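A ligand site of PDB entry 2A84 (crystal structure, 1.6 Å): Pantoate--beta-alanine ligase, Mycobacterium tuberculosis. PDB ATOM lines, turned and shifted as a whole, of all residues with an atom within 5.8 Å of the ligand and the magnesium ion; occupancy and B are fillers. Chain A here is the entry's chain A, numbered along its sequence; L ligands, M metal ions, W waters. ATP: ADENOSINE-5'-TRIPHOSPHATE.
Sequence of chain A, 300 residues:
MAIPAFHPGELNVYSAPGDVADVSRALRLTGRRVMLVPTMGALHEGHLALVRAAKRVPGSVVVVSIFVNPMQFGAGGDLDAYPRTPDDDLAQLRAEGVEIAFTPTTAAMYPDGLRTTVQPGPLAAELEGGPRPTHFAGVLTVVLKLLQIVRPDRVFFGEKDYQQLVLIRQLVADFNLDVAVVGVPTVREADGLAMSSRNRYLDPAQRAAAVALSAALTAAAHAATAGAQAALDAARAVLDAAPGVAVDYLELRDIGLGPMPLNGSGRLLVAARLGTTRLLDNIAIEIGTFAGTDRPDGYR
The backbone NH (N) of Gly 158 lies within hydrogen-bond range of an oxygen (O3') of the ligand.
The side-chain amino group (NZ) of Lys 160 is in salt-bridge range of an oxygen (O1B) of the ligand, 3.2 Å away.
The backbone carbonyl oxygen of Val 187 lies within hydrogen-bond range of a nitrogen (N6) of the ligand (2.9 Å).
The backbone NH of Val 187 is in hydrogen-bond range of a nitrogen (N1) of the ligand, at 2.9 Å.
A ring nitrogen (NE2) of His 44 lies within hydrogen-bond range of an oxygen (O1B) of the ligand (2.8 Å).
O1A of the ligand sits at hydrogen-bond distance from N of Met 40, 2.8 Å away.
The backbone carbonyl oxygen of Gly 158 lies close to an oxygen (O2') of the ligand, at 3.4 Å.
N6 of the ligand sits at hydrogen-bond distance from O of Met 195, 2.8 Å away.
N of Ser 197 sits at hydrogen-bond distance from O1B of the ligand.
The side-chain carboxylate of Asp 161 is in hydrogen-bond range of an oxygen (O2') of the ligand (2.6 Å).
The side-chain hydroxyl (OG) of Ser 196 is in hydrogen-bond range of an oxygen (O3G) of the ligand, at 2.6 Å.
An oxygen (O3G) of the ligand is in hydrogen-bond range of the backbone NH (N) of Arg 198 (2.9 Å).
NE2 of His 47 sits at hydrogen-bond distance from O3A of the ligand, 2.9 Å away.
The side-chain hydroxyl (OG) of Ser 197 lies within hydrogen-bond range of an oxygen (O3B) of the ligand, at 3.4 Å.
The guanidinium group (NE) of Arg 198 lies within salt-bridge range of an oxygen (O3G) of the ligand, 2.9 Å away.
Water W5 lies within hydrogen-bond range of the side-chain carboxylate of Asp 161 (2.7 Å) and the guanidinium group of Arg 198 (3.4 Å).
Water W9 lies within hydrogen-bond range of the side-chain carboxylate of Asp 161 (2.7 Å) and an oxygen (O5') of the ligand (3.3 Å).
Water W7 bridges O2G of the ligand (2.7 Å) and N of Arg 198 (3.3 Å).
Water W8 lies within hydrogen-bond range of an oxygen (O3') of the ligand (2.7 Å), the backbone carbonyl oxygen (O) of Pro 38 (2.7 Å) and the backbone carbonyl oxygen (O) of Phe 156 (2.8 Å).
Water W4 lies within hydrogen-bond range of O of Gly 41 (2.5 Å), OG of Ser 197 (2.8 Å), O1A of the ligand (2.9 Å) and NE2 of His 47 (3.5 Å).
No residue comes within 4 Å of the magnesium ion.
Pro 38 touches the ligand (O to C5', 3.5 Å).
Thr 39 touches the ligand (C to O1A, 3.8 Å).
Gly 46 touches the ligand (CA to C6, 3.7 Å).
CD1 of Leu 50 touches N3 of the ligand, 3.4 Å away.
Phe 157 touches the ligand (CA to O3', 3.4 Å).
Gln 164 touches the ligand (NE2 to O3', 3.9 Å).
O of Pro 185 touches C2 of the ligand, 3.6 Å away.
CA of Thr 186 touches N1 of the ligand, at 3.5 Å.
Within 4 Å of the ligand: Pro 38, Thr 39, Met 40, His 44, Gly 46, His 47, Leu 50, Phe 157, Gly 158, Lys 160, Asp 161, Gln 164, Pro 185, Thr 186, Val 187, Met 195, Ser 196, Ser 197 and Arg 198.
The nearest printed residue that does not touch the ligand is Val 184 (4.2 Å).
The backbone NH (N) of Gly 46 is in hydrogen-bond range of a ring nitrogen (ND1) of His 44.
N of Ser 197 sits at hydrogen-bond distance from NE2 of His 44, at 3.4 Å.
O of Phe 157 sits at hydrogen-bond distance from N of Val 184 (2.9 Å).
The backbone NH of Lys 160 lies within hydrogen-bond range of the side-chain hydroxyl of Thr 186.
The side-chain hydroxyl of Thr 39 lies within hydrogen-bond range of the backbone NH of Gly 41.
ND2 of Asn 199 sits close to N of Ser 196 (3.5 Å).
N of Met 195 lies within hydrogen-bond range of O of Val 187 (3.0 Å).
The backbone carbonyl oxygen (O) of Met 195 is in hydrogen-bond range of the side-chain amino group (NZ) of Lys 160 (3.1 Å).
The magnesium ion is bound by water W6 (2.0 Å), an oxygen (O2B) of the ligand (2.0 Å), water W9 (2.1 Å), an oxygen (O1G) of the ligand (2.1 Å), an oxygen (O2A) of the ligand (2.3 Å) and water W5 (2.3 Å).
The magnesium ion has six donor atoms within binding distance.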
ATOM      1  N   PRO A  38      23.547 -23.997 -18.104  1.00  0.00           N
ATOM      2  CA  PRO A  38      23.913 -25.366 -18.513  1.00  0.00           C
ATOM      3  C   PRO A  38      23.434 -26.412 -17.544  1.00  0.00           C
ATOM      4  O   PRO A  38      23.621 -26.295 -16.327  1.00  0.00           O
ATOM      5  CB  PRO A  38      25.453 -25.317 -18.539  1.00  0.00           C
ATOM      6  CG  PRO A  38      25.752 -23.843 -18.747  1.00  0.00           C
ATOM      7  CD  PRO A  38      24.754 -23.160 -17.848  1.00  0.00           C
ATOM      8  N   THR A  39      22.864 -27.489 -18.072  1.00  0.00           N
ATOM      9  CA  THR A  39      22.422 -28.602 -17.220  1.00  0.00           C
ATOM     10  C   THR A  39      22.644 -29.964 -17.904  1.00  0.00           C
ATOM     11  O   THR A  39      22.864 -30.024 -19.131  1.00  0.00           O
ATOM     12  CB  THR A  39      20.928 -28.555 -16.856  1.00  0.00           C
ATOM     13  OG1 THR A  39      20.097 -29.030 -17.961  1.00  0.00           O
ATOM     14  CG2 THR A  39      20.465 -27.151 -16.498  1.00  0.00           C
ATOM     15  N   MET A  40      22.493 -31.025 -17.103  1.00  0.00           N
ATOM     16  CA  MET A  40      22.448 -32.386 -17.652  1.00  0.00           C
ATOM     17  C   MET A  40      21.035 -32.963 -17.654  1.00  0.00           C
ATOM     18  O   MET A  40      20.840 -34.189 -17.677  1.00  0.00           O
ATOM     19  CB  MET A  40      23.412 -33.317 -16.895  1.00  0.00           C
ATOM     20  CG  MET A  40      24.770 -32.814 -16.965  1.00  0.00           C
ATOM     21  SD  MET A  40      26.016 -34.031 -16.447  1.00  0.00           S
ATOM     22  CE  MET A  40      25.607 -34.275 -14.723  1.00  0.00           C
ATOM     23  N   GLY A  41      20.025 -32.100 -17.605  1.00  0.00           N
ATOM     24  CA  GLY A  41      18.662 -32.584 -17.543  1.00  0.00           C
ATOM     25  C   GLY A  41      18.301 -33.172 -16.197  1.00  0.00           C
ATOM     26  O   GLY A  41      18.942 -32.862 -15.176  1.00  0.00           O
ATOM     27  N   HIS A  44      15.400 -30.492 -11.448  1.00  0.00           N
ATOM     28  CA  HIS A  44      14.806 -30.369 -10.114  1.00  0.00           C
ATOM     29  C   HIS A  44      14.894 -28.933  -9.647  1.00  0.00           C
ATOM     30  O   HIS A  44      15.387 -28.059 -10.375  1.00  0.00           O
ATOM     31  CB  HIS A  44      15.472 -31.299  -9.109  1.00  0.00           C
ATOM     32  CG  HIS A  44      16.934 -31.125  -9.018  1.00  0.00           C
ATOM     33  ND1 HIS A  44      17.509 -30.028  -8.412  1.00  0.00           N
ATOM     34  CD2 HIS A  44      17.950 -31.897  -9.461  1.00  0.00           C
ATOM     35  CE1 HIS A  44      18.822 -30.113  -8.531  1.00  0.00           C
ATOM     36  NE2 HIS A  44      19.112 -31.250  -9.136  1.00  0.00           N
ATOM     37  N   GLY A  46      16.739 -27.287  -7.713  1.00  0.00           N
ATOM     38  CA  GLY A  46      18.024 -26.642  -7.752  1.00  0.00           C
ATOM     39  C   GLY A  46      18.311 -26.020  -9.095  1.00  0.00           C
ATOM     40  O   GLY A  46      18.732 -24.880  -9.198  1.00  0.00           O
ATOM     41  N   HIS A  47      18.051 -26.772 -10.163  1.00  0.00           N
ATOM     42  CA  HIS A  47      18.186 -26.224 -11.502  1.00  0.00           C
ATOM     43  C   HIS A  47      17.223 -25.060 -11.671  1.00  0.00           C
ATOM     44  O   HIS A  47      17.583 -24.031 -12.301  1.00  0.00           O
ATOM     45  CB  HIS A  47      17.791 -27.238 -12.559  1.00  0.00           C
ATOM     46  CG  HIS A  47      18.602 -28.482 -12.549  1.00  0.00           C
ATOM     47  ND1 HIS A  47      18.098 -29.714 -12.210  1.00  0.00           N
ATOM     48  CD2 HIS A  47      19.906 -28.694 -12.843  1.00  0.00           C
ATOM     49  CE1 HIS A  47      19.043 -30.624 -12.308  1.00  0.00           C
ATOM     50  NE2 HIS A  47      20.151 -30.038 -12.689  1.00  0.00           N
ATOM     51  N   ALA A  49      16.200 -22.898  -9.630  1.00  0.00           N
ATOM     52  CA  ALA A  49      16.756 -21.684  -9.030  1.00  0.00           C
ATOM     53  C   ALA A  49      17.670 -20.903  -9.987  1.00  0.00           C
ATOM     54  O   ALA A  49      17.661 -19.643  -9.993  1.00  0.00           O
ATOM     55  CB  ALA A  49      17.492 -22.010  -7.731  1.00  0.00           C
ATOM     56  N   LEU A  50      18.480 -21.631 -10.760  1.00  0.00           N
ATOM     57  CA  LEU A  50      19.323 -21.005 -11.750  1.00  0.00           C
ATOM     58  C   LEU A  50      18.462 -20.385 -12.851  1.00  0.00           C
ATOM     59  O   LEU A  50      18.729 -19.247 -13.268  1.00  0.00           O
ATOM     60  CB  LEU A  50      20.327 -21.983 -12.352  1.00  0.00           C
ATOM     61  CG  LEU A  50      21.581 -22.369 -11.527  1.00  0.00           C
ATOM     62  CD1 LEU A  50      21.280 -22.980 -10.232  1.00  0.00           C
ATOM     63  CD2 LEU A  50      22.377 -23.345 -12.385  1.00  0.00           C
ATOM     64  N   PHE A 156      25.034 -19.102 -15.642  1.00  0.00           N
ATOM     65  CA  PHE A 156      24.657 -19.401 -14.249  1.00  0.00           C
ATOM     66  C   PHE A 156      25.074 -20.801 -13.866  1.00  0.00           C
ATOM     67  O   PHE A 156      24.807 -21.743 -14.616  1.00  0.00           O
ATOM     68  CB  PHE A 156      23.118 -19.310 -14.110  1.00  0.00           C
ATOM     69  CG  PHE A 156      22.611 -17.932 -14.309  1.00  0.00           C
ATOM     70  CD1 PHE A 156      22.512 -17.385 -15.592  1.00  0.00           C
ATOM     71  CD2 PHE A 156      22.340 -17.086 -13.244  1.00  0.00           C
ATOM     72  CE1 PHE A 156      22.155 -16.057 -15.793  1.00  0.00           C
ATOM     73  CE2 PHE A 156      21.968 -15.773 -13.448  1.00  0.00           C
ATOM     74  CZ  PHE A 156      21.888 -15.244 -14.714  1.00  0.00           C
ATOM     75  N   PHE A 157      25.727 -20.918 -12.697  1.00  0.00           N
ATOM     76  CA  PHE A 157      26.198 -22.173 -12.155  1.00  0.00           C
ATOM     77  C   PHE A 157      25.878 -22.228 -10.679  1.00  0.00           C
ATOM     78  O   PHE A 157      25.854 -21.195 -10.008  1.00  0.00           O
ATOM     79  CB  PHE A 157      27.705 -22.284 -12.314  1.00  0.00           C
ATOM     80  CG  PHE A 157      28.115 -22.480 -13.751  1.00  0.00           C
ATOM     81  CD1 PHE A 157      28.545 -21.465 -14.547  1.00  0.00           C
ATOM     82  CD2 PHE A 157      28.056 -23.736 -14.280  1.00  0.00           C
ATOM     83  CE1 PHE A 157      28.841 -21.731 -15.876  1.00  0.00           C
ATOM     84  CE2 PHE A 157      28.428 -23.973 -15.596  1.00  0.00           C
ATOM     85  CZ  PHE A 157      28.794 -22.965 -16.372  1.00  0.00           C
ATOM     86  N   GLY A 158      25.650 -23.416 -10.154  1.00  0.00           N
ATOM     87  CA  GLY A 158      25.319 -23.583  -8.770  1.00  0.00           C
ATOM     88  C   GLY A 158      26.512 -23.601  -7.841  1.00  0.00           C
ATOM     89  O   GLY A 158      27.556 -24.188  -8.182  1.00  0.00           O
ATOM     90  N   GLU A 159      26.391 -23.003  -6.646  1.00  0.00           N
ATOM     91  CA  GLU A 159      27.517 -23.061  -5.670  1.00  0.00           C
ATOM     92  C   GLU A 159      27.728 -24.476  -5.184  1.00  0.00           C
ATOM     93  O   GLU A 159      28.797 -24.778  -4.698  1.00  0.00           O
ATOM     94  CB  GLU A 159      27.291 -22.124  -4.496  1.00  0.00           C
ATOM     95  CG  GLU A 159      27.366 -20.678  -4.858  1.00  0.00           C
ATOM     96  CD  GLU A 159      27.238 -19.767  -3.649  1.00  0.00           C
ATOM     97  OE1 GLU A 159      27.087 -20.223  -2.504  1.00  0.00           O
ATOM     98  OE2 GLU A 159      27.417 -18.535  -3.869  1.00  0.00           O
ATOM     99  N   LYS A 160      26.716 -25.334  -5.317  1.00  0.00           N
ATOM    100  CA  LYS A 160      26.882 -26.710  -4.845  1.00  0.00           C
ATOM    101  C   LYS A 160      28.132 -27.350  -5.435  1.00  0.00           C
ATOM    102  O   LYS A 160      28.841 -28.098  -4.736  1.00  0.00           O
ATOM    103  CB  LYS A 160      25.689 -27.567  -5.259  1.00  0.00           C
ATOM    104  CG  LYS A 160      25.767 -29.024  -4.763  1.00  0.00           C
ATOM    105  CD  LYS A 160      24.613 -29.876  -5.293  1.00  0.00           C
ATOM    106  CE  LYS A 160      24.722 -30.105  -6.829  1.00  0.00           C
ATOM    107  NZ  LYS A 160      23.649 -30.999  -7.326  1.00  0.00           N
ATOM    108  N   ASP A 161      28.395 -27.081  -6.716  1.00  0.00           N
ATOM    109  CA  ASP A 161      29.604 -27.577  -7.411  1.00  0.00           C
ATOM    110  C   ASP A 161      30.622 -26.439  -7.383  1.00  0.00           C
ATOM    111  O   ASP A 161      30.881 -25.741  -8.383  1.00  0.00           O
ATOM    112  CB  ASP A 161      29.288 -28.025  -8.819  1.00  0.00           C
ATOM    113  CG  ASP A 161      28.261 -29.124  -8.832  1.00  0.00           C
ATOM    114  OD1 ASP A 161      28.646 -30.267  -8.529  1.00  0.00           O
ATOM    115  OD2 ASP A 161      27.042 -28.843  -9.062  1.00  0.00           O
ATOM    116  N   GLN A 164      33.804 -26.591  -9.522  1.00  0.00           N
ATOM    117  CA  GLN A 164      33.378 -26.321 -10.914  1.00  0.00           C
ATOM    118  C   GLN A 164      33.229 -24.819 -11.159  1.00  0.00           C
ATOM    119  O   GLN A 164      33.750 -24.262 -12.109  1.00  0.00           O
ATOM    120  CB  GLN A 164      32.073 -27.024 -11.243  1.00  0.00           C
ATOM    121  CG  GLN A 164      31.458 -26.592 -12.535  1.00  0.00           C
ATOM    122  CD  GLN A 164      30.298 -27.482 -12.893  1.00  0.00           C
ATOM    123  OE1 GLN A 164      30.511 -28.566 -13.438  1.00  0.00           O
ATOM    124  NE2 GLN A 164      29.069 -27.071 -12.455  1.00  0.00           N
ATOM    125  N   VAL A 184      24.930 -19.275  -8.077  1.00  0.00           N
ATOM    126  CA  VAL A 184      23.635 -19.255  -7.434  1.00  0.00           C
ATOM    127  C   VAL A 184      23.708 -20.140  -6.194  1.00  0.00           C
ATOM    128  O   VAL A 184      24.201 -21.288  -6.263  1.00  0.00           O
ATOM    129  CB  VAL A 184      22.593 -19.800  -8.388  1.00  0.00           C
ATOM    130  CG1 VAL A 184      21.237 -19.901  -7.784  1.00  0.00           C
ATOM    131  CG2 VAL A 184      22.494 -18.935  -9.661  1.00  0.00           C
ATOM    132  N   PRO A 185      23.222 -19.645  -5.061  1.00  0.00           N
ATOM    133  CA  PRO A 185      23.314 -20.440  -3.841  1.00  0.00           C
ATOM    134  C   PRO A 185      22.637 -21.787  -3.929  1.00  0.00           C
ATOM    135  O   PRO A 185      21.657 -21.992  -4.624  1.00  0.00           O
ATOM    136  CB  PRO A 185      22.631 -19.573  -2.802  1.00  0.00           C
ATOM    137  CG  PRO A 185      22.768 -18.160  -3.320  1.00  0.00           C
ATOM    138  CD  PRO A 185      22.693 -18.283  -4.810  1.00  0.00           C
ATOM    139  N   THR A 186      23.203 -22.704  -3.173  1.00  0.00           N
ATOM    140  CA  THR A 186      22.712 -24.081  -3.144  1.00  0.00           C
ATOM    141  C   THR A 186      21.298 -24.178  -2.580  1.00  0.00           C
ATOM    142  O   THR A 186      21.019 -23.665  -1.508  1.00  0.00           O
ATOM    143  CB  THR A 186      23.678 -24.910  -2.334  1.00  0.00           C
ATOM    144  OG1 THR A 186      24.959 -24.919  -3.024  1.00  0.00           O
ATOM    145  CG2 THR A 186      23.180 -26.352  -2.242  1.00  0.00           C
ATOM    146  N   VAL A 187      20.418 -24.841  -3.342  1.00  0.00           N
ATOM    147  CA  VAL A 187      19.039 -25.102  -2.972  1.00  0.00           C
ATOM    148  C   VAL A 187      19.027 -26.405  -2.185  1.00  0.00           C
ATOM    149  O   VAL A 187      19.628 -27.392  -2.623  1.00  0.00           O
ATOM    150  CB  VAL A 187      18.114 -25.246  -4.184  1.00  0.00           C
ATOM    151  CG1 VAL A 187      16.720 -25.482  -3.747  1.00  0.00           C
ATOM    152  CG2 VAL A 187      18.212 -23.991  -5.002  1.00  0.00           C
ATOM    153  N   ARG A 188      18.366 -26.364  -1.028  1.00  0.00           N
ATOM    154  CA  ARG A 188      18.404 -27.489  -0.095  1.00  0.00           C
ATOM    155  C   ARG A 188      16.996 -27.952   0.237  1.00  0.00           C
ATOM    156  O   ARG A 188      16.018 -27.189   0.162  1.00  0.00           O
ATOM    157  CB  ARG A 188      19.085 -27.062   1.222  1.00  0.00           C
ATOM    158  CG  ARG A 188      20.557 -26.678   1.007  1.00  0.00           C
ATOM    159  CD  ARG A 188      21.263 -26.147   2.220  1.00  0.00           C
ATOM    160  NE  ARG A 188      22.606 -25.739   1.886  1.00  0.00           N
ATOM    161  CZ  ARG A 188      23.632 -26.619   1.756  1.00  0.00           C
ATOM    162  NH1 ARG A 188      23.422 -27.909   1.928  1.00  0.00           N
ATOM    163  NH2 ARG A 188      24.845 -26.220   1.405  1.00  0.00           N
ATOM    164  N   ALA A 194      21.513 -30.921   0.176  1.00  0.00           N
ATOM    165  CA  ALA A 194      21.646 -30.247  -1.077  1.00  0.00           C
ATOM    166  C   ALA A 194      20.921 -31.007  -2.162  1.00  0.00           C
ATOM    167  O   ALA A 194      21.164 -32.176  -2.341  1.00  0.00           O
ATOM    168  CB  ALA A 194      23.060 -30.150  -1.454  1.00  0.00           C
ATOM    169  N   MET A 195      20.027 -30.350  -2.902  1.00  0.00           N
ATOM    170  CA  MET A 195      19.344 -31.067  -3.967  1.00  0.00           C
ATOM    171  C   MET A 195      20.325 -31.455  -5.064  1.00  0.00           C
ATOM    172  O   MET A 195      21.242 -30.710  -5.388  1.00  0.00           O
ATOM    173  CB  MET A 195      18.201 -30.233  -4.542  1.00  0.00           C
ATOM    174  CG  MET A 195      17.074 -30.061  -3.544  1.00  0.00           C
ATOM    175  SD  MET A 195      15.759 -29.082  -4.289  1.00  0.00           S
ATOM    176  CE  MET A 195      14.702 -28.973  -2.883  1.00  0.00           C
ATOM    177  N   SER A 196      20.116 -32.639  -5.644  1.00  0.00           N
ATOM    178  CA  SER A 196      20.988 -33.103  -6.696  1.00  0.00           C
ATOM    179  C   SER A 196      20.304 -34.236  -7.408  1.00  0.00           C
ATOM    180  O   SER A 196      19.578 -35.027  -6.762  1.00  0.00           O
ATOM    181  CB  SER A 196      22.309 -33.623  -6.125  1.00  0.00           C
ATOM    182  OG  SER A 196      23.385 -33.606  -7.083  1.00  0.00           O
ATOM    183  N   SER A 197      20.493 -34.354  -8.716  1.00  0.00           N
ATOM    184  CA  SER A 197      19.826 -35.455  -9.456  1.00  0.00           C
ATOM    185  C   SER A 197      20.172 -36.809  -8.856  1.00  0.00           C
ATOM    186  O   SER A 197      19.355 -37.734  -8.846  1.00  0.00           O
ATOM    187  CB  SER A 197      20.163 -35.385 -10.929  1.00  0.00           C
ATOM    188  OG  SER A 197      19.720 -34.107 -11.397  1.00  0.00           O
ATOM    189  N   ARG A 198      21.412 -36.938  -8.410  1.00  0.00           N
ATOM    190  CA  ARG A 198      21.902 -38.206  -7.874  1.00  0.00           C
ATOM    191  C   ARG A 198      21.204 -38.583  -6.580  1.00  0.00           C
ATOM    192  O   ARG A 198      21.290 -39.748  -6.162  1.00  0.00           O
ATOM    193  CB  ARG A 198      23.421 -38.125  -7.614  1.00  0.00           C
ATOM    194  CG  ARG A 198      23.813 -37.177  -6.582  1.00  0.00           C
ATOM    195  CD  ARG A 198      25.319 -37.042  -6.511  1.00  0.00           C
ATOM    196  NE  ARG A 198      25.826 -36.456  -7.759  1.00  0.00           N
ATOM    197  CZ  ARG A 198      27.125 -36.379  -8.072  1.00  0.00           C
ATOM    198  NH1 ARG A 198      28.028 -36.830  -7.239  1.00  0.00           N
ATOM    199  NH2 ARG A 198      27.523 -35.830  -9.206  1.00  0.00           N
ATOM    200  N   ASN A 199      20.509 -37.661  -5.916  1.00  0.00           N
ATOM    201  CA  ASN A 199      19.797 -38.014  -4.676  1.00  0.00           C
ATOM    202  C   ASN A 199      18.730 -39.081  -4.953  1.00  0.00           C
ATOM    203  O   ASN A 199      18.252 -39.800  -4.021  1.00  0.00           O
ATOM    204  CB  ASN A 199      19.125 -36.811  -4.043  1.00  0.00           C
ATOM    205  CG  ASN A 199      20.127 -35.822  -3.461  1.00  0.00           C
ATOM    206  OD1 ASN A 199      21.359 -36.037  -3.559  1.00  0.00           O
ATOM    207  ND2 ASN A 199      19.618 -34.707  -2.924  1.00  0.00           N
HETATM  208  PG  ATP L   1      24.014 -34.808 -10.609  1.00  0.00           P
HETATM  209  O1G ATP L   1      25.465 -34.356 -10.665  1.00  0.00           O
HETATM  210  O2G ATP L   1      23.756 -36.006 -11.553  1.00  0.00           O
HETATM  211  O3G ATP L   1      23.604 -35.146  -9.173  1.00  0.00           O
HETATM  212  PB  ATP L   1      23.013 -32.133 -10.553  1.00  0.00           P
HETATM  213  O1B ATP L   1      21.792 -31.985  -9.699  1.00  0.00           O
HETATM  214  O2B ATP L   1      24.361 -31.697 -10.008  1.00  0.00           O
HETATM  215  O3B ATP L   1      23.084 -33.632 -11.117  1.00  0.00           O
HETATM  216  PA  ATP L   1      23.673 -30.972 -13.110  1.00  0.00           P
HETATM  217  O1A ATP L   1      22.807 -31.005 -14.301  1.00  0.00           O
HETATM  218  O2A ATP L   1      24.897 -31.744 -12.923  1.00  0.00           O
HETATM  219  O3A ATP L   1      22.655 -31.320 -11.887  1.00  0.00           O
HETATM  220  O5' ATP L   1      23.972 -29.426 -12.757  1.00  0.00           O
HETATM  221  C5' ATP L   1      23.528 -28.336 -13.547  1.00  0.00           C
HETATM  222  C4' ATP L   1      23.744 -27.031 -12.802  1.00  0.00           C
HETATM  223  O4' ATP L   1      22.730 -26.986 -11.746  1.00  0.00           O
HETATM  224  C3' ATP L   1      25.101 -26.872 -12.144  1.00  0.00           C
HETATM  225  O3' ATP L   1      25.504 -25.508 -12.225  1.00  0.00           O
HETATM  226  C2' ATP L   1      24.807 -27.208 -10.676  1.00  0.00           C
HETATM  227  O2' ATP L   1      25.750 -26.641  -9.767  1.00  0.00           O
HETATM  228  C1' ATP L   1      23.416 -26.639 -10.580  1.00  0.00           C
HETATM  229  N9  ATP L   1      22.748 -27.240  -9.409  1.00  0.00           N
HETATM  230  C8  ATP L   1      22.470 -28.557  -9.228  1.00  0.00           C
HETATM  231  N7  ATP L   1      21.881 -28.746  -7.975  1.00  0.00           N
HETATM  232  C5  ATP L   1      21.830 -27.517  -7.413  1.00  0.00           C
HETATM  233  C6  ATP L   1      21.376 -27.027  -6.148  1.00  0.00           C
HETATM  234  N6  ATP L   1      20.868 -27.903  -5.242  1.00  0.00           N
HETATM  235  N1  ATP L   1      21.466 -25.718  -5.954  1.00  0.00           N
HETATM  236  C2  ATP L   1      21.982 -24.841  -6.839  1.00  0.00           C
HETATM  237  N3  ATP L   1      22.461 -25.229  -7.998  1.00  0.00           N
HETATM  238  C4  ATP L   1      22.408 -26.542  -8.326  1.00  0.00           C
HETATM  239 MG    MG M   1      25.957 -32.315 -11.005  1.00  0.00          MG
HETATM  240  O   HOH W   1      28.094 -35.544 -12.593  1.00  0.00           O
HETATM  241  O   HOH W   2      25.898 -37.151 -12.650  1.00  0.00           O
HETATM  242  O   HOH W   3      22.336 -35.670 -13.870  1.00  0.00           O
HETATM  243  O   HOH W   4      20.984 -33.230 -13.752  1.00  0.00           O
HETATM  244  O   HOH W   5      27.153 -32.419  -9.057  1.00  0.00           O
HETATM  245  O   HOH W   6      27.434 -32.934 -12.133  1.00  0.00           O
HETATM  246  O   HOH W   7      22.437 -38.294 -11.265  1.00  0.00           O
HETATM  247  O   HOH W   8      24.972 -24.585 -14.672  1.00  0.00           O
HETATM  248  O   HOH W   9      26.746 -30.373 -11.229  1.00  0.00           O
